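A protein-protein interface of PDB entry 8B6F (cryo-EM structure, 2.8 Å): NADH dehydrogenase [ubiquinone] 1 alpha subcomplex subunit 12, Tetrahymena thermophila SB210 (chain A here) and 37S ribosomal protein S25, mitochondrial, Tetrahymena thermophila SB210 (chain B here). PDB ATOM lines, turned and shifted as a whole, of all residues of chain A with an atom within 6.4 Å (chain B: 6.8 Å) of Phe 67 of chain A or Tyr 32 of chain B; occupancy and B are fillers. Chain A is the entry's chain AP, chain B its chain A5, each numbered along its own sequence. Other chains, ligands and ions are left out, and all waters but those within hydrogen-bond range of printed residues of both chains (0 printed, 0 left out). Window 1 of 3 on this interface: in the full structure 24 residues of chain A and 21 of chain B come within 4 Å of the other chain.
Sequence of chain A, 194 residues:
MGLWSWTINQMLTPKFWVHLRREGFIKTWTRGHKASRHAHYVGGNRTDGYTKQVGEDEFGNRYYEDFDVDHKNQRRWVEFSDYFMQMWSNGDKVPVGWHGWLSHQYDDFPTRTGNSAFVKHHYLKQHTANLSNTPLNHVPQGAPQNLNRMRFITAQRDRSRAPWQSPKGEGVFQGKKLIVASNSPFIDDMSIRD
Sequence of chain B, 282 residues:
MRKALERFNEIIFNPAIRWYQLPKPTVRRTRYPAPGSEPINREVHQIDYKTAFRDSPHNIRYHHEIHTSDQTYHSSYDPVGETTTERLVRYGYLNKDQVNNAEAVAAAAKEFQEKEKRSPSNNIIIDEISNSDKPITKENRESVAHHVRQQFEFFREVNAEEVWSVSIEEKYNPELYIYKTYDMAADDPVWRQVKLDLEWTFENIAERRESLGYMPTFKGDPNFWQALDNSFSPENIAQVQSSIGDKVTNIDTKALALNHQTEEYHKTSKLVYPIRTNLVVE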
ATOM      1  N   THR A  51      -3.824 -24.434   5.230  1.00  0.00           N
ATOM      2  CA  THR A  51      -3.829 -23.413   6.267  1.00  0.00           C
ATOM      3  C   THR A  51      -2.416 -23.141   6.761  1.00  0.00           C
ATOM      4  O   THR A  51      -1.624 -24.062   6.970  1.00  0.00           O
ATOM      5  CB  THR A  51      -4.710 -23.856   7.437  1.00  0.00           C
ATOM      6  OG1 THR A  51      -6.021 -24.179   6.958  1.00  0.00           O
ATOM      7  CG2 THR A  51      -4.819 -22.755   8.479  1.00  0.00           C
ATOM      8  N   GLU A  65      -5.528 -22.657  12.401  1.00  0.00           N
ATOM      9  CA  GLU A  65      -6.838 -22.020  12.488  1.00  0.00           C
ATOM     10  C   GLU A  65      -7.357 -21.792  11.078  1.00  0.00           C
ATOM     11  O   GLU A  65      -6.710 -21.103  10.284  1.00  0.00           O
ATOM     12  CB  GLU A  65      -6.766 -20.699  13.256  1.00  0.00           C
ATOM     13  CG  GLU A  65      -8.112 -20.013  13.414  1.00  0.00           C
ATOM     14  CD  GLU A  65      -8.031 -18.760  14.260  1.00  0.00           C
ATOM     15  OE1 GLU A  65      -6.903 -18.341  14.591  1.00  0.00           O
ATOM     16  OE2 GLU A  65      -9.092 -18.196  14.596  1.00  0.00           O
ATOM     17  N   ASP A  66      -8.520 -22.366  10.770  1.00  0.00           N
ATOM     18  CA  ASP A  66      -9.154 -22.221   9.467  1.00  0.00           C
ATOM     19  C   ASP A  66     -10.569 -21.700   9.660  1.00  0.00           C
ATOM     20  O   ASP A  66     -11.322 -22.238  10.477  1.00  0.00           O
ATOM     21  CB  ASP A  66      -9.177 -23.556   8.714  1.00  0.00           C
ATOM     22  CG  ASP A  66      -9.757 -23.431   7.318  1.00  0.00           C
ATOM     23  OD1 ASP A  66     -10.118 -22.306   6.916  1.00  0.00           O
ATOM     24  OD2 ASP A  66      -9.851 -24.461   6.619  1.00  0.00           O
ATOM     25  N   PHE A  67     -10.928 -20.664   8.907  1.00  0.00           N
ATOM     26  CA  PHE A  67     -12.241 -20.043   9.012  1.00  0.00           C
ATOM     27  C   PHE A  67     -13.249 -20.585   8.006  1.00  0.00           C
ATOM     28  O   PHE A  67     -14.391 -20.117   7.989  1.00  0.00           O
ATOM     29  CB  PHE A  67     -12.118 -18.525   8.837  1.00  0.00           C
ATOM     30  CG  PHE A  67     -11.511 -17.828  10.017  1.00  0.00           C
ATOM     31  CD1 PHE A  67     -10.136 -17.725  10.147  1.00  0.00           C
ATOM     32  CD2 PHE A  67     -12.316 -17.275  10.999  1.00  0.00           C
ATOM     33  CE1 PHE A  67      -9.576 -17.084  11.233  1.00  0.00           C
ATOM     34  CE2 PHE A  67     -11.763 -16.633  12.086  1.00  0.00           C
ATOM     35  CZ  PHE A  67     -10.390 -16.537  12.204  1.00  0.00           C
ATOM     36  N   ASP A  68     -12.864 -21.548   7.171  1.00  0.00           N
ATOM     37  CA  ASP A  68     -13.767 -22.135   6.191  1.00  0.00           C
ATOM     38  C   ASP A  68     -14.326 -23.479   6.636  1.00  0.00           C
ATOM     39  O   ASP A  68     -14.971 -24.165   5.838  1.00  0.00           O
ATOM     40  CB  ASP A  68     -13.061 -22.287   4.842  1.00  0.00           C
ATOM     41  CG  ASP A  68     -12.968 -20.980   4.085  1.00  0.00           C
ATOM     42  OD1 ASP A  68     -13.282 -19.925   4.675  1.00  0.00           O
ATOM     43  OD2 ASP A  68     -12.601 -21.007   2.893  1.00  0.00           O
ATOM     44  N   VAL A  69     -14.093 -23.875   7.888  1.00  0.00           N
ATOM     45  CA  VAL A  69     -14.680 -25.110   8.386  1.00  0.00           C
ATOM     46  C   VAL A  69     -16.201 -24.988   8.366  1.00  0.00           C
ATOM     47  O   VAL A  69     -16.766 -23.899   8.517  1.00  0.00           O
ATOM     48  CB  VAL A  69     -14.171 -25.437   9.800  1.00  0.00           C
ATOM     49  CG1 VAL A  69     -12.700 -25.804   9.757  1.00  0.00           C
ATOM     50  CG2 VAL A  69     -14.401 -24.263  10.741  1.00  0.00           C
ATOM     51  N   ARG A  75     -12.800 -24.316  14.141  1.00  0.00           N
ATOM     52  CA  ARG A  75     -11.845 -23.396  13.525  1.00  0.00           C
ATOM     53  C   ARG A  75     -10.411 -23.763  13.889  1.00  0.00           C
ATOM     54  O   ARG A  75      -9.541 -23.853  13.017  1.00  0.00           O
ATOM     55  CB  ARG A  75     -12.141 -21.957  13.948  1.00  0.00           C
ATOM     56  CG  ARG A  75     -13.455 -21.402  13.431  1.00  0.00           C
ATOM     57  CD  ARG A  75     -13.401 -19.885  13.345  1.00  0.00           C
ATOM     58  NE  ARG A  75     -12.809 -19.291  14.539  1.00  0.00           N
ATOM     59  CZ  ARG A  75     -13.486 -18.945  15.625  1.00  0.00           C
ATOM     60  NH1 ARG A  75     -14.794 -19.118  15.711  1.00  0.00           N
ATOM     61  NH2 ARG A  75     -12.833 -18.409  16.651  1.00  0.00           N
ATOM     62  N   ARG A  76     -10.150 -23.985  15.174  1.00  0.00           N
ATOM     63  CA  ARG A  76      -8.799 -24.163  15.690  1.00  0.00           C
ATOM     64  C   ARG A  76      -8.575 -25.629  16.026  1.00  0.00           C
ATOM     65  O   ARG A  76      -9.430 -26.261  16.655  1.00  0.00           O
ATOM     66  CB  ARG A  76      -8.577 -23.294  16.928  1.00  0.00           C
ATOM     67  CG  ARG A  76      -8.778 -21.811  16.672  1.00  0.00           C
ATOM     68  CD  ARG A  76      -8.684 -21.000  17.953  1.00  0.00           C
ATOM     69  NE  ARG A  76      -8.836 -19.573  17.694  1.00  0.00           N
ATOM     70  CZ  ARG A  76      -8.870 -18.638  18.632  1.00  0.00           C
ATOM     71  NH1 ARG A  76      -8.772 -18.943  19.915  1.00  0.00           N
ATOM     72  NH2 ARG A  76      -9.009 -17.366  18.276  1.00  0.00           N
ATOM     73  N   HIS A 104     -10.725 -21.163  23.003  1.00  0.00           N
ATOM     74  CA  HIS A 104     -11.327 -19.915  22.548  1.00  0.00           C
ATOM     75  C   HIS A 104     -11.628 -18.976  23.709  1.00  0.00           C
ATOM     76  O   HIS A 104     -12.576 -18.191  23.649  1.00  0.00           O
ATOM     77  CB  HIS A 104     -12.598 -20.166  21.731  1.00  0.00           C
ATOM     78  CG  HIS A 104     -12.350 -20.852  20.425  1.00  0.00           C
ATOM     79  ND1 HIS A 104     -12.268 -22.223  20.308  1.00  0.00           N
ATOM     80  CD2 HIS A 104     -12.167 -20.357  19.180  1.00  0.00           C
ATOM     81  CE1 HIS A 104     -12.047 -22.542  19.045  1.00  0.00           C
ATOM     82  NE2 HIS A 104     -11.981 -21.428  18.340  1.00  0.00           N
ATOM     83  N   ASP A 107      -8.112 -14.727  21.851  1.00  0.00           N
ATOM     84  CA  ASP A 107      -7.569 -14.882  20.509  1.00  0.00           C
ATOM     85  C   ASP A 107      -6.058 -14.697  20.452  1.00  0.00           C
ATOM     86  O   ASP A 107      -5.486 -14.746  19.360  1.00  0.00           O
ATOM     87  CB  ASP A 107      -8.246 -13.896  19.554  1.00  0.00           C
ATOM     88  CG  ASP A 107      -9.740 -14.141  19.428  1.00  0.00           C
ATOM     89  OD1 ASP A 107     -10.173 -15.294  19.630  1.00  0.00           O
ATOM     90  OD2 ASP A 107     -10.479 -13.182  19.126  1.00  0.00           O
ATOM     91  N   VAL B  27     -17.435 -10.144   8.246  1.00  0.00           N
ATOM     92  CA  VAL B  27     -17.237  -9.130   9.276  1.00  0.00           C
ATOM     93  C   VAL B  27     -17.730  -9.625  10.629  1.00  0.00           C
ATOM     94  O   VAL B  27     -17.199  -9.230  11.673  1.00  0.00           O
ATOM     95  CB  VAL B  27     -17.936  -7.812   8.894  1.00  0.00           C
ATOM     96  CG1 VAL B  27     -17.419  -7.302   7.561  1.00  0.00           C
ATOM     97  CG2 VAL B  27     -19.450  -7.988   8.850  1.00  0.00           C
ATOM     98  N   ARG B  28     -18.748 -10.482  10.630  1.00  0.00           N
ATOM     99  CA  ARG B  28     -19.421 -10.901  11.852  1.00  0.00           C
ATOM    100  C   ARG B  28     -19.320 -12.409  12.022  1.00  0.00           C
ATOM    101  O   ARG B  28     -19.664 -13.167  11.109  1.00  0.00           O
ATOM    102  CB  ARG B  28     -20.891 -10.465  11.831  1.00  0.00           C
ATOM    103  CG  ARG B  28     -21.747 -11.034  12.954  1.00  0.00           C
ATOM    104  CD  ARG B  28     -21.189 -10.705  14.327  1.00  0.00           C
ATOM    105  NE  ARG B  28     -22.070 -11.177  15.388  1.00  0.00           N
ATOM    106  CZ  ARG B  28     -21.774 -11.150  16.680  1.00  0.00           C
ATOM    107  NH1 ARG B  28     -20.612 -10.692  17.114  1.00  0.00           N
ATOM    108  NH2 ARG B  28     -22.667 -11.594  17.560  1.00  0.00           N
ATOM    109  N   ARG B  29     -18.848 -12.835  13.191  1.00  0.00           N
ATOM    110  CA  ARG B  29     -18.856 -14.232  13.596  1.00  0.00           C
ATOM    111  C   ARG B  29     -19.423 -14.322  15.003  1.00  0.00           C
ATOM    112  O   ARG B  29     -19.444 -13.340  15.750  1.00  0.00           O
ATOM    113  CB  ARG B  29     -17.455 -14.855  13.545  1.00  0.00           C
ATOM    114  CG  ARG B  29     -16.827 -14.883  12.160  1.00  0.00           C
ATOM    115  CD  ARG B  29     -17.620 -15.758  11.204  1.00  0.00           C
ATOM    116  NE  ARG B  29     -17.006 -15.819   9.882  1.00  0.00           N
ATOM    117  CZ  ARG B  29     -16.130 -16.737   9.496  1.00  0.00           C
ATOM    118  NH1 ARG B  29     -15.732 -17.700  10.309  1.00  0.00           N
ATOM    119  NH2 ARG B  29     -15.641 -16.685   8.261  1.00  0.00           N
ATOM    120  N   THR B  30     -19.889 -15.518  15.362  1.00  0.00           N
ATOM    121  CA  THR B  30     -20.661 -15.669  16.592  1.00  0.00           C
ATOM    122  C   THR B  30     -19.834 -15.320  17.824  1.00  0.00           C
ATOM    123  O   THR B  30     -20.251 -14.503  18.653  1.00  0.00           O
ATOM    124  CB  THR B  30     -21.204 -17.092  16.705  1.00  0.00           C
ATOM    125  OG1 THR B  30     -20.120 -17.998  16.936  1.00  0.00           O
ATOM    126  CG2 THR B  30     -21.906 -17.487  15.419  1.00  0.00           C
ATOM    127  N   ARG B  31     -18.658 -15.931  17.964  1.00  0.00           N
ATOM    128  CA  ARG B  31     -17.811 -15.739  19.136  1.00  0.00           C
ATOM    129  C   ARG B  31     -16.485 -15.075  18.789  1.00  0.00           C
ATOM    130  O   ARG B  31     -15.531 -15.161  19.567  1.00  0.00           O
ATOM    131  CB  ARG B  31     -17.564 -17.075  19.839  1.00  0.00           C
ATOM    132  CG  ARG B  31     -18.628 -17.444  20.863  1.00  0.00           C
ATOM    133  CD  ARG B  31     -18.371 -18.822  21.448  1.00  0.00           C
ATOM    134  NE  ARG B  31     -17.010 -18.953  21.960  1.00  0.00           N
ATOM    135  CZ  ARG B  31     -16.641 -18.696  23.207  1.00  0.00           C
ATOM    136  NH1 ARG B  31     -17.511 -18.294  24.119  1.00  0.00           N
ATOM    137  NH2 ARG B  31     -15.365 -18.846  23.549  1.00  0.00           N
ATOM    138  N   TYR B  32     -16.402 -14.414  17.637  1.00  0.00           N
ATOM    139  CA  TYR B  32     -15.185 -13.735  17.224  1.00  0.00           C
ATOM    140  C   TYR B  32     -15.389 -12.234  17.356  1.00  0.00           C
ATOM    141  O   TYR B  32     -16.302 -11.686  16.719  1.00  0.00           O
ATOM    142  CB  TYR B  32     -14.820 -14.102  15.788  1.00  0.00           C
ATOM    143  CG  TYR B  32     -13.338 -14.066  15.503  1.00  0.00           C
ATOM    144  CD1 TYR B  32     -12.477 -14.987  16.086  1.00  0.00           C
ATOM    145  CD2 TYR B  32     -12.802 -13.128  14.633  1.00  0.00           C
ATOM    146  CE1 TYR B  32     -11.124 -14.965  15.821  1.00  0.00           C
ATOM    147  CE2 TYR B  32     -11.448 -13.098  14.362  1.00  0.00           C
ATOM    148  CZ  TYR B  32     -10.614 -14.019  14.959  1.00  0.00           C
ATOM    149  OH  TYR B  32      -9.265 -13.995  14.693  1.00  0.00           O
ATOM    150  N   PRO B  33     -14.585 -11.524  18.158  1.00  0.00           N
ATOM    151  CA  PRO B  33     -13.453 -12.020  18.957  1.00  0.00           C
ATOM    152  C   PRO B  33     -13.900 -12.826  20.167  1.00  0.00           C
ATOM    153  O   PRO B  33     -15.039 -12.733  20.609  1.00  0.00           O
ATOM    154  CB  PRO B  33     -12.731 -10.729  19.366  1.00  0.00           C
ATOM    155  CG  PRO B  33     -13.804  -9.692  19.395  1.00  0.00           C
ATOM    156  CD  PRO B  33     -14.758 -10.067  18.296  1.00  0.00           C
ATOM    157  N   ALA B  34     -12.998 -13.630  20.718  1.00  0.00           N
ATOM    158  CA  ALA B  34     -13.323 -14.457  21.860  1.00  0.00           C
ATOM    159  C   ALA B  34     -13.554 -13.589  23.092  1.00  0.00           C
ATOM    160  O   ALA B  34     -13.111 -12.440  23.145  1.00  0.00           O
ATOM    161  CB  ALA B  34     -12.203 -15.457  22.126  1.00  0.00           C
ATOM    162  N   SER B  37     -10.730 -11.505  24.413  1.00  0.00           N
ATOM    163  CA  SER B  37     -10.248 -10.419  23.569  1.00  0.00           C
ATOM    164  C   SER B  37     -11.346  -9.448  23.154  1.00  0.00           C
ATOM    165  O   SER B  37     -11.106  -8.587  22.303  1.00  0.00           O
ATOM    166  CB  SER B  37      -9.562 -10.989  22.327  1.00  0.00           C
ATOM    167  OG  SER B  37     -10.448 -11.813  21.593  1.00  0.00           O
ATOM    168  N   GLU B  38     -12.542  -9.560  23.723  1.00  0.00           N
ATOM    169  CA  GLU B  38     -13.611  -8.642  23.368  1.00  0.00           C
ATOM    170  C   GLU B  38     -13.297  -7.238  23.882  1.00  0.00           C
ATOM    171  O   GLU B  38     -12.645  -7.078  24.916  1.00  0.00           O
ATOM    172  CB  GLU B  38     -14.940  -9.115  23.944  1.00  0.00           C
ATOM    173  CG  GLU B  38     -15.582 -10.248  23.168  1.00  0.00           C
ATOM    174  CD  GLU B  38     -16.817 -10.791  23.853  1.00  0.00           C
ATOM    175  OE1 GLU B  38     -17.173 -10.274  24.931  1.00  0.00           O
ATOM    176  OE2 GLU B  38     -17.428 -11.739  23.316  1.00  0.00           O
ATOM    177  N   ARG B 209     -20.981  -2.801  11.599  1.00  0.00           N
ATOM    178  CA  ARG B 209     -19.603  -3.266  11.710  1.00  0.00           C
ATOM    179  C   ARG B 209     -18.862  -3.135  10.385  1.00  0.00           C
ATOM    180  O   ARG B 209     -17.692  -2.738  10.361  1.00  0.00           O
ATOM    181  CB  ARG B 209     -19.575  -4.710  12.206  1.00  0.00           C
ATOM    182  CG  ARG B 209     -20.087  -4.861  13.626  1.00  0.00           C
ATOM    183  CD  ARG B 209     -19.703  -6.198  14.227  1.00  0.00           C
ATOM    184  NE  ARG B 209     -20.197  -6.326  15.591  1.00  0.00           N
ATOM    185  CZ  ARG B 209     -19.870  -7.308  16.420  1.00  0.00           C
ATOM    186  NH1 ARG B 209     -19.037  -8.269  16.057  1.00  0.00           N
ATOM    187  NH2 ARG B 209     -20.388  -7.323  17.644  1.00  0.00           N
ATOM    188  N   MET B 215     -12.527  -3.835  14.223  1.00  0.00           N
ATOM    189  CA  MET B 215     -13.049  -4.148  15.546  1.00  0.00           C
ATOM    190  C   MET B 215     -11.949  -4.000  16.593  1.00  0.00           C
ATOM    191  O   MET B 215     -10.951  -4.726  16.539  1.00  0.00           O
ATOM    192  CB  MET B 215     -13.608  -5.571  15.564  1.00  0.00           C
ATOM    193  CG  MET B 215     -14.317  -5.964  16.848  1.00  0.00           C
ATOM    194  SD  MET B 215     -15.869  -5.086  17.072  1.00  0.00           S
ATOM    195  CE  MET B 215     -16.516  -5.929  18.507  1.00  0.00           C
ATOM    196  N   LEU B 271      -8.948  -6.078  15.023  1.00  0.00           N
ATOM    197  CA  LEU B 271      -9.328  -7.131  14.091  1.00  0.00           C
ATOM    198  C   LEU B 271      -9.842  -6.471  12.818  1.00  0.00           C
ATOM    199  O   LEU B 271     -10.848  -5.756  12.849  1.00  0.00           O
ATOM    200  CB  LEU B 271     -10.391  -8.041  14.704  1.00  0.00           C
ATOM    201  CG  LEU B 271     -10.990  -9.105  13.782  1.00  0.00           C
ATOM    202  CD1 LEU B 271      -9.935 -10.120  13.369  1.00  0.00           C
ATOM    203  CD2 LEU B 271     -12.165  -9.790  14.455  1.00  0.00           C
ATOM    204  N   TYR B 273     -11.378  -6.414   9.103  1.00  0.00           N
ATOM    205  CA  TYR B 273     -12.200  -7.140   8.156  1.00  0.00           C
ATOM    206  C   TYR B 273     -11.590  -7.057   6.759  1.00  0.00           C
ATOM    207  O   TYR B 273     -10.827  -6.137   6.457  1.00  0.00           O
ATOM    208  CB  TYR B 273     -13.617  -6.572   8.143  1.00  0.00           C
ATOM    209  CG  TYR B 273     -14.276  -6.523   9.503  1.00  0.00           C
ATOM    210  CD1 TYR B 273     -13.967  -7.459  10.483  1.00  0.00           C
ATOM    211  CD2 TYR B 273     -15.202  -5.537   9.810  1.00  0.00           C
ATOM    212  CE1 TYR B 273     -14.566  -7.417  11.726  1.00  0.00           C
ATOM    213  CE2 TYR B 273     -15.806  -5.486  11.051  1.00  0.00           C
ATOM    214  CZ  TYR B 273     -15.483  -6.429  12.005  1.00  0.00           C
ATOM    215  OH  TYR B 273     -16.082  -6.383  13.241  1.00  0.00           O
ATOM    216  N   ILE B 275     -12.738 -11.184   7.513  1.00  0.00           N
ATOM    217  CA  ILE B 275     -12.137 -12.338   8.173  1.00  0.00           C
ATOM    218  C   ILE B 275     -11.880 -13.405   7.118  1.00  0.00           C
ATOM    219  O   ILE B 275     -12.799 -13.822   6.405  1.00  0.00           O
ATOM    220  CB  ILE B 275     -13.043 -12.867   9.293  1.00  0.00           C
ATOM    221  CG1 ILE B 275     -13.282 -11.776  10.341  1.00  0.00           C
ATOM    222  CG2 ILE B 275     -12.420 -14.088   9.949  1.00  0.00           C
ATOM    223  CD1 ILE B 275     -14.378 -12.106  11.334  1.00  0.00           C
ATOM    224  N   ARG B 276     -10.630 -13.850   7.016  1.00  0.00           N
ATOM    225  CA  ARG B 276     -10.257 -14.837   6.014  1.00  0.00           C
ATOM    226  C   ARG B 276      -9.189 -15.753   6.590  1.00  0.00           C
ATOM    227  O   ARG B 276      -8.483 -15.401   7.538  1.00  0.00           O
ATOM    228  CB  ARG B 276      -9.757 -14.169   4.728  1.00  0.00           C
ATOM    229  CG  ARG B 276      -8.606 -13.202   4.943  1.00  0.00           C
ATOM    230  CD  ARG B 276      -8.112 -12.628   3.626  1.00  0.00           C
ATOM    231  NE  ARG B 276      -7.563 -13.661   2.755  1.00  0.00           N
ATOM    232  CZ  ARG B 276      -6.324 -14.129   2.829  1.00  0.00           C
ATOM    233  NH1 ARG B 276      -5.468 -13.680   3.732  1.00  0.00           N
ATOM    234  NH2 ARG B 276      -5.935 -15.073   1.978  1.00  0.00           N
ATOM    235  N   THR B 277      -9.081 -16.942   6.002  1.00  0.00           N
ATOM    236  CA  THR B 277      -8.104 -17.925   6.443  1.00  0.00           C
ATOM    237  C   THR B 277      -6.757 -17.663   5.782  1.00  0.00           C
ATOM    238  O   THR B 277      -6.686 -17.426   4.573  1.00  0.00           O
ATOM    239  CB  THR B 277      -8.578 -19.338   6.104  1.00  0.00           C
ATOM    240  OG1 THR B 277      -9.853 -19.583   6.710  1.00  0.00           O
ATOM    241  CG2 THR B 277      -7.580 -20.375   6.602  1.00  0.00           C
ATOM    242  N   ASN B 278      -5.693 -17.698   6.579  1.00  0.00           N
ATOM    243  CA  ASN B 278      -4.349 -17.614   6.027  1.00  0.00           C
ATOM    244  C   ASN B 278      -4.013 -18.904   5.294  1.00  0.00           C
ATOM    245  O   ASN B 278      -4.208 -20.000   5.828  1.00  0.00           O
ATOM    246  CB  ASN B 278      -3.334 -17.356   7.138  1.00  0.00           C
ATOM    247  CG  ASN B 278      -3.590 -16.057   7.867  1.00  0.00           C
ATOM    248  OD1 ASN B 278      -3.916 -16.050   9.054  1.00  0.00           O
ATOM    249  ND2 ASN B 278      -3.441 -14.944   7.158  1.00  0.00           N
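OD1 of Asp 66 of chain A sits at hydrogen-bond distance from OG1 of Thr 277 of chain B (2.7 Å).
N of Phe 67 of chain A is in hydrogen-bond range of OG1 of Thr 277 of chain B (2.7 Å).
The backbone carbonyl oxygen (O) of His 104 of chain A is in hydrogen-bond range of the guanidinium group (NH2) of Arg 31 of chain B (2.9 Å).
The backbone NH (N) of Ala 34 of chain B lies within hydrogen-bond range of the side-chain carboxylate (OD2) of Asp 107 of chain A (3.0 Å).
The side-chain carboxylate (OD2) of Asp 107 of chain A is in hydrogen-bond range of the side-chain hydroxyl (OG) of Ser 37 of chain B (2.8 Å).
The side-chain carboxylate (OE2) of Glu 65 of chain A is in salt-bridge range of the guanidinium group (NE) of Arg 75 of chain A (3.9 Å).
OE2 of Glu 65 of chain A is in salt-bridge range of NE of Arg 76 of chain A.
OD1 of Asp 66 of chain A is in hydrogen-bond range of N of Asp 68 of chain A.
The backbone NH (N) of Asp 66 of chain A lies within hydrogen-bond range of the backbone carbonyl oxygen (O) of Arg 75 of chain A.
The guanidinium group (NH2) of Arg 76 of chain A is in salt-bridge range of the side-chain carboxylate (OD1) of Asp 107 of chain A (2.7 Å).
The backbone carbonyl oxygen (O) of Ala 34 of chain B lies within hydrogen-bond range of the side-chain hydroxyl (OG) of Ser 37 of chain B (3.1 Å).
Among the printed residues, pairs that only touch across the chains: Thr 51 of chain A with Asn 278 of chain B, Glu 65 of chain A with Thr 277 of chain B, Phe 67 of chain A with Arg 29 of chain B, Phe 67 of chain A with Tyr 32 of chain B, Phe 67 of chain A with Ile 275 of chain B, Phe 67 of chain A with Arg 276 of chain B, Asp 68 of chain A with Thr 277 of chain B, Arg 75 of chain A with Tyr 32 of chain B, His 104 of chain A with Ala 34 of chain B, Asp 107 of chain A with Tyr 32 of chain B and Asp 107 of chain A with Pro 33 of chain B.
Printed residues of chain B within 4 Å of Asp 66 of chain A: Thr 277 (2.7 Å).
Of chain B, only Arg 29 (3.5 Å), Tyr 32 (3.7 Å), Ile 275 (3.4 Å), Arg 276 (3.9 Å) and Thr 277 (2.7 Å) come within 4 Å of Phe 67 of chain A.
Printed residues of chain B within 4 Å of Arg 75 of chain A: Tyr 32 (3.5 Å).
Of the printed residues of chain A, Tyr 32 of chain B touches Phe 67, Arg 75 and Asp 107.
Of the printed residues of chain A, Ala 34 of chain B touches His 104 and Asp 107.
The nearest residue of chain B that does not touch Phe 67 of chain A is Asn 278 of chain B (5.7 Å).
The nearest printed residue of chain A that does not touch Tyr 32 of chain B is Glu 65 of chain A (4.01 Å).
Printed residues of chain B that touch a printed residue of chain A: Arg 29, Arg 31, Tyr 32, Pro 33, Ala 34, Ser 37, Ile 275, Arg 276, Thr 277 and Asn 278.
Hydrophobic or aromatic side chains of chain B that line the printed part of chain A: Tyr 32, Pro 33, Ala 34 and Ile 275.
Among the printed residues, 16 pairs touch across the chains.
Among the printed residues, no Asp or Glu carboxylate lies within 4 Å of a Lys or Arg side-chain nitrogen of the other chain.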
